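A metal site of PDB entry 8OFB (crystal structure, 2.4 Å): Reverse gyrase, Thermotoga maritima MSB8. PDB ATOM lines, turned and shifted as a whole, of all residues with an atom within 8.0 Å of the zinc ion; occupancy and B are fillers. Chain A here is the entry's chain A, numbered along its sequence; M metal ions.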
ATOM      1  N   ARG A 559     -26.750  26.783  27.930  1.00  0.00           N
ATOM      2  CA  ARG A 559     -27.587  25.682  27.473  1.00  0.00           C
ATOM      3  C   ARG A 559     -27.851  25.848  25.989  1.00  0.00           C
ATOM      4  O   ARG A 559     -28.340  26.891  25.560  1.00  0.00           O
ATOM      5  CB  ARG A 559     -28.907  25.623  28.251  1.00  0.00           C
ATOM      6  CG  ARG A 559     -29.796  24.445  27.868  1.00  0.00           C
ATOM      7  CD  ARG A 559     -31.154  24.533  28.534  1.00  0.00           C
ATOM      8  NE  ARG A 559     -31.889  25.719  28.111  1.00  0.00           N
ATOM      9  CZ  ARG A 559     -32.697  25.773  27.051  1.00  0.00           C
ATOM     10  NH1 ARG A 559     -32.884  24.715  26.285  1.00  0.00           N
ATOM     11  NH2 ARG A 559     -33.318  26.911  26.766  1.00  0.00           N
ATOM     12  N   CYS A 560     -27.518  24.823  25.217  1.00  0.00           N
ATOM     13  CA  CYS A 560     -27.841  24.823  23.802  1.00  0.00           C
ATOM     14  C   CYS A 560     -29.336  24.593  23.623  1.00  0.00           C
ATOM     15  O   CYS A 560     -29.901  23.649  24.191  1.00  0.00           O
ATOM     16  CB  CYS A 560     -27.047  23.740  23.068  1.00  0.00           C
ATOM     17  SG  CYS A 560     -27.404  23.599  21.307  1.00  0.00           S
ATOM     18  N   ARG A 561     -29.987  25.459  22.843  1.00  0.00           N
ATOM     19  CA  ARG A 561     -31.426  25.340  22.664  1.00  0.00           C
ATOM     20  C   ARG A 561     -31.808  24.274  21.635  1.00  0.00           C
ATOM     21  O   ARG A 561     -32.993  23.922  21.545  1.00  0.00           O
ATOM     22  CB  ARG A 561     -32.037  26.686  22.257  1.00  0.00           C
ATOM     23  CG  ARG A 561     -31.939  27.752  23.340  1.00  0.00           C
ATOM     24  CD  ARG A 561     -32.820  28.951  22.998  1.00  0.00           C
ATOM     25  NE  ARG A 561     -32.655  30.039  23.957  1.00  0.00           N
ATOM     26  CZ  ARG A 561     -31.817  31.054  23.795  1.00  0.00           C
ATOM     27  NH1 ARG A 561     -31.041  31.144  22.720  1.00  0.00           N
ATOM     28  NH2 ARG A 561     -31.746  31.988  24.726  1.00  0.00           N
ATOM     29  N   ASP A 562     -30.850  23.764  20.860  1.00  0.00           N
ATOM     30  CA  ASP A 562     -31.135  22.755  19.858  1.00  0.00           C
ATOM     31  C   ASP A 562     -31.065  21.344  20.449  1.00  0.00           C
ATOM     32  O   ASP A 562     -32.037  20.582  20.369  1.00  0.00           O
ATOM     33  CB  ASP A 562     -30.174  22.897  18.676  1.00  0.00           C
ATOM     34  CG  ASP A 562     -30.314  24.222  17.964  1.00  0.00           C
ATOM     35  OD1 ASP A 562     -31.112  25.062  18.421  1.00  0.00           O
ATOM     36  OD2 ASP A 562     -29.625  24.431  16.940  1.00  0.00           O
ATOM     37  N   CYS A 563     -29.926  20.985  21.034  1.00  0.00           N
ATOM     38  CA  CYS A 563     -29.716  19.653  21.579  1.00  0.00           C
ATOM     39  C   CYS A 563     -29.837  19.583  23.089  1.00  0.00           C
ATOM     40  O   CYS A 563     -29.916  18.482  23.643  1.00  0.00           O
ATOM     41  CB  CYS A 563     -28.348  19.114  21.155  1.00  0.00           C
ATOM     42  SG  CYS A 563     -26.953  19.829  22.043  1.00  0.00           S
ATOM     43  N   GLY A 564     -29.848  20.727  23.780  1.00  0.00           N
ATOM     44  CA  GLY A 564     -30.029  20.754  25.210  1.00  0.00           C
ATOM     45  C   GLY A 564     -28.780  20.534  26.037  1.00  0.00           C
ATOM     46  O   GLY A 564     -28.866  20.498  27.273  1.00  0.00           O
ATOM     47  N   TYR A 565     -27.613  20.393  25.401  1.00  0.00           N
ATOM     48  CA  TYR A 565     -26.379  20.182  26.147  1.00  0.00           C
ATOM     49  C   TYR A 565     -26.019  21.428  26.942  1.00  0.00           C
ATOM     50  O   TYR A 565     -26.167  22.562  26.466  1.00  0.00           O
ATOM     51  CB  TYR A 565     -25.245  19.831  25.184  1.00  0.00           C
ATOM     52  CG  TYR A 565     -24.005  19.270  25.854  1.00  0.00           C
ATOM     53  CD1 TYR A 565     -23.980  17.962  26.309  1.00  0.00           C
ATOM     54  CD2 TYR A 565     -22.867  20.043  26.008  1.00  0.00           C
ATOM     55  CE1 TYR A 565     -22.857  17.440  26.920  1.00  0.00           C
ATOM     56  CE2 TYR A 565     -21.735  19.530  26.615  1.00  0.00           C
ATOM     57  CZ  TYR A 565     -21.730  18.222  27.069  1.00  0.00           C
ATOM     58  OH  TYR A 565     -20.608  17.709  27.676  1.00  0.00           O
ATOM     59  N   GLN A 566     -25.548  21.219  28.175  1.00  0.00           N
ATOM     60  CA  GLN A 566     -25.199  22.312  29.069  1.00  0.00           C
ATOM     61  C   GLN A 566     -23.703  22.289  29.370  1.00  0.00           C
ATOM     62  O   GLN A 566     -23.080  21.220  29.438  1.00  0.00           O
ATOM     63  CB  GLN A 566     -25.990  22.241  30.386  1.00  0.00           C
ATOM     64  CG  GLN A 566     -27.423  22.737  30.266  1.00  0.00           C
ATOM     65  CD  GLN A 566     -28.113  22.866  31.612  1.00  0.00           C
ATOM     66  OE1 GLN A 566     -27.759  22.186  32.572  1.00  0.00           O
ATOM     67  NE2 GLN A 566     -29.099  23.763  31.679  1.00  0.00           N
ATOM     68  N   PHE A 567     -23.142  23.484  29.546  1.00  0.00           N
ATOM     69  CA  PHE A 567     -21.707  23.642  29.762  1.00  0.00           C
ATOM     70  C   PHE A 567     -21.471  25.018  30.381  1.00  0.00           C
ATOM     71  O   PHE A 567     -22.351  25.883  30.371  1.00  0.00           O
ATOM     72  CB  PHE A 567     -20.929  23.479  28.459  1.00  0.00           C
ATOM     73  CG  PHE A 567     -21.391  24.386  27.347  1.00  0.00           C
ATOM     74  CD1 PHE A 567     -22.484  24.048  26.568  1.00  0.00           C
ATOM     75  CD2 PHE A 567     -20.733  25.578  27.094  1.00  0.00           C
ATOM     76  CE1 PHE A 567     -22.919  24.875  25.548  1.00  0.00           C
ATOM     77  CE2 PHE A 567     -21.158  26.406  26.074  1.00  0.00           C
ATOM     78  CZ  PHE A 567     -22.252  26.063  25.308  1.00  0.00           C
ATOM     79  N   GLU A 573     -20.167  28.377  20.228  1.00  0.00           N
ATOM     80  CA  GLU A 573     -20.927  27.271  19.659  1.00  0.00           C
ATOM     81  C   GLU A 573     -21.011  26.121  20.649  1.00  0.00           C
ATOM     82  O   GLU A 573     -20.191  25.990  21.558  1.00  0.00           O
ATOM     83  CB  GLU A 573     -20.307  26.784  18.344  1.00  0.00           C
ATOM     84  CG  GLU A 573     -20.283  27.829  17.241  1.00  0.00           C
ATOM     85  CD  GLU A 573     -19.713  27.286  15.947  1.00  0.00           C
ATOM     86  OE1 GLU A 573     -19.176  26.153  15.971  1.00  0.00           O
ATOM     87  OE2 GLU A 573     -19.803  27.983  14.923  1.00  0.00           O
ATOM     88  N   CYS A 574     -22.034  25.300  20.460  1.00  0.00           N
ATOM     89  CA  CYS A 574     -22.239  24.135  21.316  1.00  0.00           C
ATOM     90  C   CYS A 574     -21.120  23.124  21.113  1.00  0.00           C
ATOM     91  O   CYS A 574     -20.739  22.835  19.977  1.00  0.00           O
ATOM     92  CB  CYS A 574     -23.593  23.496  21.022  1.00  0.00           C
ATOM     93  SG  CYS A 574     -23.967  22.036  22.006  1.00  0.00           S
ATOM     94  N   PRO A 575     -20.568  22.567  22.199  1.00  0.00           N
ATOM     95  CA  PRO A 575     -19.492  21.565  22.042  1.00  0.00           C
ATOM     96  C   PRO A 575     -19.948  20.278  21.356  1.00  0.00           C
ATOM     97  O   PRO A 575     -19.100  19.536  20.849  1.00  0.00           O
ATOM     98  CB  PRO A 575     -19.042  21.305  23.483  1.00  0.00           C
ATOM     99  CG  PRO A 575     -19.531  22.476  24.267  1.00  0.00           C
ATOM    100  CD  PRO A 575     -20.807  22.888  23.605  1.00  0.00           C
ATOM    101  N   VAL A 576     -21.250  20.004  21.322  1.00  0.00           N
ATOM    102  CA  VAL A 576     -21.757  18.744  20.796  1.00  0.00           C
ATOM    103  C   VAL A 576     -22.182  18.907  19.334  1.00  0.00           C
ATOM    104  O   VAL A 576     -21.663  18.217  18.450  1.00  0.00           O
ATOM    105  CB  VAL A 576     -22.925  18.212  21.639  1.00  0.00           C
ATOM    106  CG1 VAL A 576     -23.515  16.967  21.002  1.00  0.00           C
ATOM    107  CG2 VAL A 576     -22.452  17.909  23.057  1.00  0.00           C
ATOM    108  N   CYS A 577     -23.118  19.823  19.068  1.00  0.00           N
ATOM    109  CA  CYS A 577     -23.682  19.989  17.737  1.00  0.00           C
ATOM    110  C   CYS A 577     -23.209  21.251  17.023  1.00  0.00           C
ATOM    111  O   CYS A 577     -23.649  21.509  15.901  1.00  0.00           O
ATOM    112  CB  CYS A 577     -25.210  19.979  17.809  1.00  0.00           C
ATOM    113  SG  CYS A 577     -25.916  21.346  18.743  1.00  0.00           S
ATOM    114  N   SER A 578     -22.332  22.045  17.650  1.00  0.00           N
ATOM    115  CA  SER A 578     -21.762  23.242  17.038  1.00  0.00           C
ATOM    116  C   SER A 578     -22.827  24.283  16.685  1.00  0.00           C
ATOM    117  O   SER A 578     -22.663  25.053  15.725  1.00  0.00           O
ATOM    118  CB  SER A 578     -20.921  22.890  15.801  1.00  0.00           C
ATOM    119  OG  SER A 578     -19.926  21.930  16.113  1.00  0.00           O
ATOM    120  N   SER A 579     -23.918  24.323  17.438  1.00  0.00           N
ATOM    121  CA  SER A 579     -24.979  25.299  17.212  1.00  0.00           C
ATOM    122  C   SER A 579     -24.689  26.585  17.973  1.00  0.00           C
ATOM    123  O   SER A 579     -24.176  26.567  19.094  1.00  0.00           O
ATOM    124  CB  SER A 579     -26.331  24.740  17.649  1.00  0.00           C
ATOM    125  OG  SER A 579     -27.347  25.709  17.507  1.00  0.00           O
ATOM    126  N   LYS A 580     -25.018  27.715  17.343  1.00  0.00           N
ATOM    127  CA  LYS A 580     -24.829  29.027  17.964  1.00  0.00           C
ATOM    128  C   LYS A 580     -26.028  29.485  18.776  1.00  0.00           C
ATOM    129  O   LYS A 580     -25.944  30.513  19.449  1.00  0.00           O
ATOM    130  CB  LYS A 580     -24.487  30.068  16.899  1.00  0.00           C
ATOM    131  CG  LYS A 580     -23.163  29.846  16.201  1.00  0.00           C
ATOM    132  CD  LYS A 580     -22.866  30.945  15.194  1.00  0.00           C
ATOM    133  CE  LYS A 580     -21.514  30.740  14.534  1.00  0.00           C
ATOM    134  NZ  LYS A 580     -21.224  31.778  13.510  1.00  0.00           N
ATOM    135  N   ASN A 581     -27.144  28.757  18.725  1.00  0.00           N
ATOM    136  CA  ASN A 581     -28.346  29.107  19.487  1.00  0.00           C
ATOM    137  C   ASN A 581     -28.147  28.618  20.909  1.00  0.00           C
ATOM    138  O   ASN A 581     -28.534  27.498  21.273  1.00  0.00           O
ATOM    139  CB  ASN A 581     -29.588  28.497  18.837  1.00  0.00           C
ATOM    140  CG  ASN A 581     -30.868  28.914  19.530  1.00  0.00           C
ATOM    141  OD1 ASN A 581     -30.897  29.898  20.279  1.00  0.00           O
ATOM    142  ND2 ASN A 581     -31.941  28.161  19.296  1.00  0.00           N
ATOM    143  N   ILE A 582     -27.556  29.468  21.742  1.00  0.00           N
ATOM    144  CA  ILE A 582     -27.158  29.107  23.103  1.00  0.00           C
ATOM    145  C   ILE A 582     -27.822  30.065  24.076  1.00  0.00           C
ATOM    146  O   ILE A 582     -27.771  31.295  23.891  1.00  0.00           O
ATOM    147  CB  ILE A 582     -25.625  29.145  23.270  1.00  0.00           C
ATOM    148  CG1 ILE A 582     -24.961  28.183  22.287  1.00  0.00           C
ATOM    149  CG2 ILE A 582     -25.242  28.802  24.698  1.00  0.00           C
ATOM    150  CD1 ILE A 582     -23.451  28.180  22.361  1.00  0.00           C
HETATM  151 ZN    ZN M   1     -26.062  21.721  21.041  1.00  0.00          ZN
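N of Cys 574 sits at hydrogen-bond distance from O of Ser 579, 2.8 Å away.
The backbone NH (N) of Tyr 565 lies close to the side-chain sulfur (SG) of Cys 563, 3.5 Å away.
The side-chain sulfur of Cys 574 lies close to the backbone NH of Val 576 (3.5 Å).
The side-chain sulfur (SG) of Cys 560 sits close to the backbone NH (N) of Asp 562.
The backbone NH (N) of Cys 560 lies within hydrogen-bond range of the backbone carbonyl oxygen (O) of Tyr 565 (2.9 Å).
Of the 19 residues printed, 4 come within 4 Å of the zinc ion.
The side-chain sulfur (SG) of Cys 563 is bound to the zinc ion.
The zinc ion is bound by SG of Cys 560, at 2.3 Å.
The side-chain sulfur (SG) of Cys 574 binds the zinc ion (2.3 Å).
SG of Cys 577 binds the zinc ion, 2.3 Å away.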
